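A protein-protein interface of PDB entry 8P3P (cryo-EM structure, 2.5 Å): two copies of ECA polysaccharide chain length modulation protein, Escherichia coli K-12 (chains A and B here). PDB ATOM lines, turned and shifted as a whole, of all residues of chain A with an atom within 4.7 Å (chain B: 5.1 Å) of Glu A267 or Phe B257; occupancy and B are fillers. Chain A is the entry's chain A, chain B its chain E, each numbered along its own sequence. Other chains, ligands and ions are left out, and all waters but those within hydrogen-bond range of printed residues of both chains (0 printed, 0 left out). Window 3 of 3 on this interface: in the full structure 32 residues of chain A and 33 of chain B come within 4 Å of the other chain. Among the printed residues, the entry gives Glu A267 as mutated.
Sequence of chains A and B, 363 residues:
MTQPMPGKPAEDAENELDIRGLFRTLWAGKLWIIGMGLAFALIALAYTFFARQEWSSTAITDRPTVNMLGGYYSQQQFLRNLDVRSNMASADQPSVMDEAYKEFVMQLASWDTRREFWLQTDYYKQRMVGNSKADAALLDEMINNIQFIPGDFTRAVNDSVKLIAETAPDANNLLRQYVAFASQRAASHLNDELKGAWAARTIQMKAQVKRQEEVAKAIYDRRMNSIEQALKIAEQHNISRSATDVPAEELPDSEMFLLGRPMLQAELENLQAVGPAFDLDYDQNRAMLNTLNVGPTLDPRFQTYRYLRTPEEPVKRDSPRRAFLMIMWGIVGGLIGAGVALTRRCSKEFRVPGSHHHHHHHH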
ATOM      1  N   ARG A 223     -20.990  27.006   6.538  1.00  0.00           N
ATOM      2  CA  ARG A 223     -20.994  26.810   5.090  1.00  0.00           C
ATOM      3  C   ARG A 223     -20.155  25.599   4.688  1.00  0.00           C
ATOM      4  O   ARG A 223     -20.546  24.832   3.799  1.00  0.00           O
ATOM      5  CB  ARG A 223     -20.496  28.069   4.385  1.00  0.00           C
ATOM      6  CG  ARG A 223     -20.785  28.089   2.897  1.00  0.00           C
ATOM      7  CD  ARG A 223     -20.884  29.512   2.373  1.00  0.00           C
ATOM      8  NE  ARG A 223     -20.129  29.698   1.141  1.00  0.00           N
ATOM      9  CZ  ARG A 223     -20.512  29.257  -0.050  1.00  0.00           C
ATOM     10  NH1 ARG A 223     -21.651  28.602  -0.211  1.00  0.00           N
ATOM     11  NH2 ARG A 223     -19.737  29.481  -1.106  1.00  0.00           N
ATOM     12  N   ILE A 227     -21.579  22.308   2.673  1.00  0.00           N
ATOM     13  CA  ILE A 227     -20.988  21.810   1.434  1.00  0.00           C
ATOM     14  C   ILE A 227     -20.530  20.367   1.589  1.00  0.00           C
ATOM     15  O   ILE A 227     -20.737  19.545   0.688  1.00  0.00           O
ATOM     16  CB  ILE A 227     -19.833  22.720   0.977  1.00  0.00           C
ATOM     17  CG1 ILE A 227     -20.355  24.117   0.644  1.00  0.00           C
ATOM     18  CG2 ILE A 227     -19.128  22.123  -0.227  1.00  0.00           C
ATOM     19  CD1 ILE A 227     -19.272  25.089   0.254  1.00  0.00           C
ATOM     20  N   MET A 263     -18.561  20.287  -9.412  1.00  0.00           N
ATOM     21  CA  MET A 263     -18.865  21.638  -8.956  1.00  0.00           C
ATOM     22  C   MET A 263     -18.809  21.737  -7.437  1.00  0.00           C
ATOM     23  O   MET A 263     -18.291  22.718  -6.891  1.00  0.00           O
ATOM     24  CB  MET A 263     -20.235  22.072  -9.474  1.00  0.00           C
ATOM     25  CG  MET A 263     -20.299  22.607 -10.919  1.00  0.00           C
ATOM     26  SD  MET A 263     -18.930  23.593 -11.591  1.00  0.00           S
ATOM     27  CE  MET A 263     -17.678  22.371 -12.005  1.00  0.00           C
ATOM     28  N   LEU A 264     -19.337  20.732  -6.736  1.00  0.00           N
ATOM     29  CA  LEU A 264     -19.299  20.756  -5.277  1.00  0.00           C
ATOM     30  C   LEU A 264     -17.868  20.679  -4.761  1.00  0.00           C
ATOM     31  O   LEU A 264     -17.508  21.385  -3.812  1.00  0.00           O
ATOM     32  CB  LEU A 264     -20.138  19.614  -4.711  1.00  0.00           C
ATOM     33  CG  LEU A 264     -21.636  19.895  -4.573  1.00  0.00           C
ATOM     34  CD1 LEU A 264     -22.332  18.756  -3.852  1.00  0.00           C
ATOM     35  CD2 LEU A 264     -21.872  21.212  -3.855  1.00  0.00           C
ATOM     36  N   GLN A 265     -17.035  19.833  -5.371  1.00  0.00           N
ATOM     37  CA  GLN A 265     -15.640  19.745  -4.953  1.00  0.00           C
ATOM     38  C   GLN A 265     -14.903  21.051  -5.216  1.00  0.00           C
ATOM     39  O   GLN A 265     -14.101  21.500  -4.386  1.00  0.00           O
ATOM     40  CB  GLN A 265     -14.950  18.586  -5.672  1.00  0.00           C
ATOM     41  CG  GLN A 265     -13.526  18.336  -5.217  1.00  0.00           C
ATOM     42  CD  GLN A 265     -13.436  18.034  -3.736  1.00  0.00           C
ATOM     43  OE1 GLN A 265     -12.668  18.663  -3.008  1.00  0.00           O
ATOM     44  NE2 GLN A 265     -14.221  17.067  -3.280  1.00  0.00           N
ATOM     45  N   ALA A 266     -15.156  21.675  -6.369  1.00  0.00           N
ATOM     46  CA  ALA A 266     -14.522  22.953  -6.669  1.00  0.00           C
ATOM     47  C   ALA A 266     -14.959  24.028  -5.684  1.00  0.00           C
ATOM     48  O   ALA A 266     -14.137  24.836  -5.234  1.00  0.00           O
ATOM     49  CB  ALA A 266     -14.840  23.371  -8.103  1.00  0.00           C
ATOM     50  N   GLU A 267     -16.247  24.055  -5.336  1.00  0.00           N
ATOM     51  CA  GLU A 267     -16.726  25.013  -4.345  1.00  0.00           C
ATOM     52  C   GLU A 267     -16.082  24.768  -2.989  1.00  0.00           C
ATOM     53  O   GLU A 267     -15.705  25.716  -2.290  1.00  0.00           O
ATOM     54  CB  GLU A 267     -18.248  24.935  -4.233  1.00  0.00           C
ATOM     55  CG  GLU A 267     -18.860  26.011  -3.356  1.00  0.00           C
ATOM     56  CD  GLU A 267     -20.367  25.900  -3.267  1.00  0.00           C
ATOM     57  OE1 GLU A 267     -20.933  24.976  -3.887  1.00  0.00           O
ATOM     58  OE2 GLU A 267     -20.987  26.736  -2.577  1.00  0.00           O
ATOM     59  N   LEU A 268     -15.951  23.499  -2.599  1.00  0.00           N
ATOM     60  CA  LEU A 268     -15.315  23.168  -1.330  1.00  0.00           C
ATOM     61  C   LEU A 268     -13.874  23.658  -1.304  1.00  0.00           C
ATOM     62  O   LEU A 268     -13.434  24.286  -0.333  1.00  0.00           O
ATOM     63  CB  LEU A 268     -15.385  21.656  -1.104  1.00  0.00           C
ATOM     64  CG  LEU A 268     -15.091  21.068   0.278  1.00  0.00           C
ATOM     65  CD1 LEU A 268     -13.601  20.869   0.513  1.00  0.00           C
ATOM     66  CD2 LEU A 268     -15.696  21.945   1.355  1.00  0.00           C
ATOM     67  N   GLU A 269     -13.126  23.393  -2.378  1.00  0.00           N
ATOM     68  CA  GLU A 269     -11.732  23.822  -2.433  1.00  0.00           C
ATOM     69  C   GLU A 269     -11.616  25.341  -2.434  1.00  0.00           C
ATOM     70  O   GLU A 269     -10.743  25.905  -1.764  1.00  0.00           O
ATOM     71  CB  GLU A 269     -11.051  23.230  -3.666  1.00  0.00           C
ATOM     72  CG  GLU A 269     -10.963  21.715  -3.650  1.00  0.00           C
ATOM     73  CD  GLU A 269      -9.966  21.180  -4.654  1.00  0.00           C
ATOM     74  OE1 GLU A 269      -9.755  21.839  -5.692  1.00  0.00           O
ATOM     75  OE2 GLU A 269      -9.392  20.098  -4.406  1.00  0.00           O
ATOM     76  N   ASN A 270     -12.488  26.022  -3.180  1.00  0.00           N
ATOM     77  CA  ASN A 270     -12.441  27.479  -3.233  1.00  0.00           C
ATOM     78  C   ASN A 270     -12.753  28.094  -1.875  1.00  0.00           C
ATOM     79  O   ASN A 270     -12.089  29.049  -1.454  1.00  0.00           O
ATOM     80  CB  ASN A 270     -13.411  27.994  -4.293  1.00  0.00           C
ATOM     81  CG  ASN A 270     -13.264  29.478  -4.544  1.00  0.00           C
ATOM     82  OD1 ASN A 270     -12.190  30.046  -4.357  1.00  0.00           O
ATOM     83  ND2 ASN A 270     -14.346  30.115  -4.973  1.00  0.00           N
ATOM     84  N   LEU A 271     -13.760  27.565  -1.176  1.00  0.00           N
ATOM     85  CA  LEU A 271     -14.085  28.083   0.147  1.00  0.00           C
ATOM     86  C   LEU A 271     -12.970  27.791   1.142  1.00  0.00           C
ATOM     87  O   LEU A 271     -12.680  28.617   2.016  1.00  0.00           O
ATOM     88  CB  LEU A 271     -15.411  27.496   0.630  1.00  0.00           C
ATOM     89  CG  LEU A 271     -15.892  27.952   2.008  1.00  0.00           C
ATOM     90  CD1 LEU A 271     -15.990  29.463   2.076  1.00  0.00           C
ATOM     91  CD2 LEU A 271     -17.227  27.319   2.338  1.00  0.00           C
ATOM     92  N   ALA B 230      -9.192  31.444  -6.891  1.00  0.00           N
ATOM     93  CA  ALA B 230     -10.247  30.935  -7.758  1.00  0.00           C
ATOM     94  C   ALA B 230      -9.698  30.556  -9.126  1.00  0.00           C
ATOM     95  O   ALA B 230     -10.088  29.533  -9.697  1.00  0.00           O
ATOM     96  CB  ALA B 230     -11.364  31.969  -7.895  1.00  0.00           C
ATOM     97  N   ILE B 233      -7.805  27.262  -8.773  1.00  0.00           N
ATOM     98  CA  ILE B 233      -8.722  26.138  -8.618  1.00  0.00           C
ATOM     99  C   ILE B 233      -9.402  25.813  -9.943  1.00  0.00           C
ATOM    100  O   ILE B 233      -9.560  24.641 -10.304  1.00  0.00           O
ATOM    101  CB  ILE B 233      -9.744  26.430  -7.502  1.00  0.00           C
ATOM    102  CG1 ILE B 233      -9.308  25.769  -6.193  1.00  0.00           C
ATOM    103  CG2 ILE B 233     -11.134  25.944  -7.887  1.00  0.00           C
ATOM    104  CD1 ILE B 233      -7.979  26.259  -5.664  1.00  0.00           C
ATOM    105  N   ALA B 234      -9.809  26.841 -10.693  1.00  0.00           N
ATOM    106  CA  ALA B 234     -10.454  26.611 -11.981  1.00  0.00           C
ATOM    107  C   ALA B 234      -9.500  25.950 -12.966  1.00  0.00           C
ATOM    108  O   ALA B 234      -9.901  25.062 -13.726  1.00  0.00           O
ATOM    109  CB  ALA B 234     -10.984  27.927 -12.547  1.00  0.00           C
ATOM    110  N   ILE B 239     -12.068  24.083 -15.513  1.00  0.00           N
ATOM    111  CA  ILE B 239     -13.343  24.783 -15.689  1.00  0.00           C
ATOM    112  C   ILE B 239     -13.058  25.938 -16.643  1.00  0.00           C
ATOM    113  O   ILE B 239     -12.800  27.068 -16.232  1.00  0.00           O
ATOM    114  CB  ILE B 239     -13.931  25.257 -14.362  1.00  0.00           C
ATOM    115  CG1 ILE B 239     -14.029  24.095 -13.374  1.00  0.00           C
ATOM    116  CG2 ILE B 239     -15.306  25.876 -14.583  1.00  0.00           C
ATOM    117  CD1 ILE B 239     -14.438  24.521 -11.981  1.00  0.00           C
ATOM    118  N   SER B 254     -15.915  33.495  -2.064  1.00  0.00           N
ATOM    119  CA  SER B 254     -15.962  32.040  -2.012  1.00  0.00           C
ATOM    120  C   SER B 254     -16.652  31.427  -3.222  1.00  0.00           C
ATOM    121  O   SER B 254     -16.473  30.232  -3.480  1.00  0.00           O
ATOM    122  CB  SER B 254     -16.668  31.583  -0.736  1.00  0.00           C
ATOM    123  OG  SER B 254     -17.910  32.247  -0.576  1.00  0.00           O
ATOM    124  N   GLU B 255     -17.433  32.211  -3.965  1.00  0.00           N
ATOM    125  CA  GLU B 255     -18.163  31.716  -5.125  1.00  0.00           C
ATOM    126  C   GLU B 255     -17.558  32.181  -6.442  1.00  0.00           C
ATOM    127  O   GLU B 255     -18.185  32.017  -7.493  1.00  0.00           O
ATOM    128  CB  GLU B 255     -19.630  32.142  -5.046  1.00  0.00           C
ATOM    129  CG  GLU B 255     -20.506  31.199  -4.240  1.00  0.00           C
ATOM    130  CD  GLU B 255     -21.713  31.895  -3.646  1.00  0.00           C
ATOM    131  OE1 GLU B 255     -22.458  32.548  -4.406  1.00  0.00           O
ATOM    132  OE2 GLU B 255     -21.918  31.790  -2.418  1.00  0.00           O
ATOM    133  N   MET B 256     -16.355  32.756  -6.415  1.00  0.00           N
ATOM    134  CA  MET B 256     -15.737  33.253  -7.635  1.00  0.00           C
ATOM    135  C   MET B 256     -15.257  32.137  -8.550  1.00  0.00           C
ATOM    136  O   MET B 256     -14.895  32.415  -9.698  1.00  0.00           O
ATOM    137  CB  MET B 256     -14.571  34.179  -7.291  1.00  0.00           C
ATOM    138  CG  MET B 256     -15.003  35.506  -6.699  1.00  0.00           C
ATOM    139  SD  MET B 256     -14.293  36.918  -7.558  1.00  0.00           S
ATOM    140  CE  MET B 256     -15.441  37.095  -8.920  1.00  0.00           C
ATOM    141  N   PHE B 257     -15.242  30.890  -8.077  1.00  0.00           N
ATOM    142  CA  PHE B 257     -14.822  29.773  -8.912  1.00  0.00           C
ATOM    143  C   PHE B 257     -15.804  29.468 -10.033  1.00  0.00           C
ATOM    144  O   PHE B 257     -15.433  28.764 -10.978  1.00  0.00           O
ATOM    145  CB  PHE B 257     -14.628  28.519  -8.061  1.00  0.00           C
ATOM    146  CG  PHE B 257     -15.900  27.770  -7.801  1.00  0.00           C
ATOM    147  CD1 PHE B 257     -16.833  28.257  -6.903  1.00  0.00           C
ATOM    148  CD2 PHE B 257     -16.171  26.589  -8.468  1.00  0.00           C
ATOM    149  CE1 PHE B 257     -18.006  27.572  -6.665  1.00  0.00           C
ATOM    150  CE2 PHE B 257     -17.343  25.902  -8.238  1.00  0.00           C
ATOM    151  CZ  PHE B 257     -18.262  26.394  -7.337  1.00  0.00           C
ATOM    152  N   LEU B 258     -17.036  29.975  -9.962  1.00  0.00           N
ATOM    153  CA  LEU B 258     -18.021  29.684 -10.996  1.00  0.00           C
ATOM    154  C   LEU B 258     -17.803  30.583 -12.204  1.00  0.00           C
ATOM    155  O   LEU B 258     -18.745  31.201 -12.710  1.00  0.00           O
ATOM    156  CB  LEU B 258     -19.442  29.862 -10.458  1.00  0.00           C
ATOM    157  CG  LEU B 258     -19.880  28.969  -9.301  1.00  0.00           C
ATOM    158  CD1 LEU B 258     -20.890  29.691  -8.426  1.00  0.00           C
ATOM    159  CD2 LEU B 258     -20.459  27.667  -9.825  1.00  0.00           C
ATOM    160  N   LEU B 259     -16.564  30.640 -12.678  1.00  0.00           N
ATOM    161  CA  LEU B 259     -16.196  31.388 -13.869  1.00  0.00           C
ATOM    162  C   LEU B 259     -15.030  30.667 -14.523  1.00  0.00           C
ATOM    163  O   LEU B 259     -14.190  30.075 -13.841  1.00  0.00           O
ATOM    164  CB  LEU B 259     -15.813  32.839 -13.549  1.00  0.00           C
ATOM    165  CG  LEU B 259     -16.871  33.765 -12.944  1.00  0.00           C
ATOM    166  CD1 LEU B 259     -16.235  35.036 -12.409  1.00  0.00           C
ATOM    167  CD2 LEU B 259     -17.945  34.092 -13.967  1.00  0.00           C
ATOM    168  N   LEU B 264     -12.099  34.555 -15.492  1.00  0.00           N
ATOM    169  CA  LEU B 264     -11.366  34.871 -14.270  1.00  0.00           C
ATOM    170  C   LEU B 264     -10.121  35.697 -14.572  1.00  0.00           C
ATOM    171  O   LEU B 264      -9.804  36.640 -13.840  1.00  0.00           O
ATOM    172  CB  LEU B 264     -10.998  33.587 -13.530  1.00  0.00           C
ATOM    173  CG  LEU B 264     -12.122  32.970 -12.696  1.00  0.00           C
ATOM    174  CD1 LEU B 264     -11.617  31.780 -11.904  1.00  0.00           C
ATOM    175  CD2 LEU B 264     -12.727  34.010 -11.770  1.00  0.00           C
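The guanidinium group (NH2) of Arg A223 is in salt-bridge range of the side-chain carboxylate (OE2) of Glu B255 (3.4 Å).
The guanidinium group of Arg A223 lies within hydrogen-bond range of the side-chain hydroxyl of Ser B254, 3.4 Å away.
ND2 of Asn A270 is in hydrogen-bond range of O of Ser B254, 2.6 Å away.
The side-chain amide nitrogen (ND2) of Asn A270 lies close to the backbone NH (N) of Phe B257.
Among the printed residues, pairs that only touch across the chains: Met A263 with Ile B239, Met A263 with Phe B257, Ala A266 with Phe B257, Glu A267 with Phe B257, Glu A269 with Ile B233, Asn A270 with Glu B255, Asn A270 with Met B256 and Leu A271 with Ser B254.
Printed residues of chain B that touch a printed residue of chain A: Ile B233, Ile B239, Ser B254, Glu B255, Met B256 and Phe B257.
Hydrophobic or aromatic side chains of chain B within 4 Å of the printed part of chain A: Ile B233, Ile B239 and Phe B257.
Of the 11 printed residues of chain A, 7 touch a printed residue of chain B.
Printed residues of chain A that touch a printed residue of chain B: Arg A223, Met A263, Ala A266, Glu A267, Glu A269, Asn A270 and Leu A271.
Hydrophobic or aromatic side chains of chain A within 4 Å of the printed part of chain B: Met A263, Ala A266 and Leu A271.
Along chain A the printed residues that touch a printed residue of chain B span positions 223 to 271.
Among the printed residues, 12 pairs touch across the chains.
Among the printed residues, Asp or Glu carboxylates within 4 Å of a Lys or Arg side-chain nitrogen of the other chain: Arg A223 with Glu B255.
Position printed for both chains: 264.
Of the 12 pairs that touch across the chains among the printed residues, none has its exchanged pair printed and touching as well.
The side-chain carboxylate (OE2) of Glu A267 lies within salt-bridge range of the guanidinium group (NH1) of Arg A223 (3.1 Å).
The backbone NH (N) of Ile B239 sits at hydrogen-bond distance from the backbone carbonyl oxygen (O) of Ala B234, at 3.0 Å.
Of the printed residues of chain B, Arg A223 touches Ser B254 (3.4 Å) and Glu B255 (3.4 Å).
Of the printed residues of chain B, Met A263 touches Ile B239 and Phe B257.
Of the printed residues of chain B, Ala A266 touches Phe B257.
Glu A267 touches just one residue of chain B: Phe B257 (3.4 Å).
Of the printed residues of chain B, Glu A269 touches Ile B233 (3.98 Å).
Ala B230 touches none of the printed residues of chain A.
Of the printed residues of chain A, Ser B254 touches Arg A223 (3.4 Å), Asn A270 (2.6 Å) and Leu A271 (3.6 Å).
Phe B257 touches just these residues of chain A: Met A263, Ala A266, Glu A267 and Asn A270.
The nearest printed residue of chain A that does not touch Met B256 is Arg A223 (7.1 Å).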
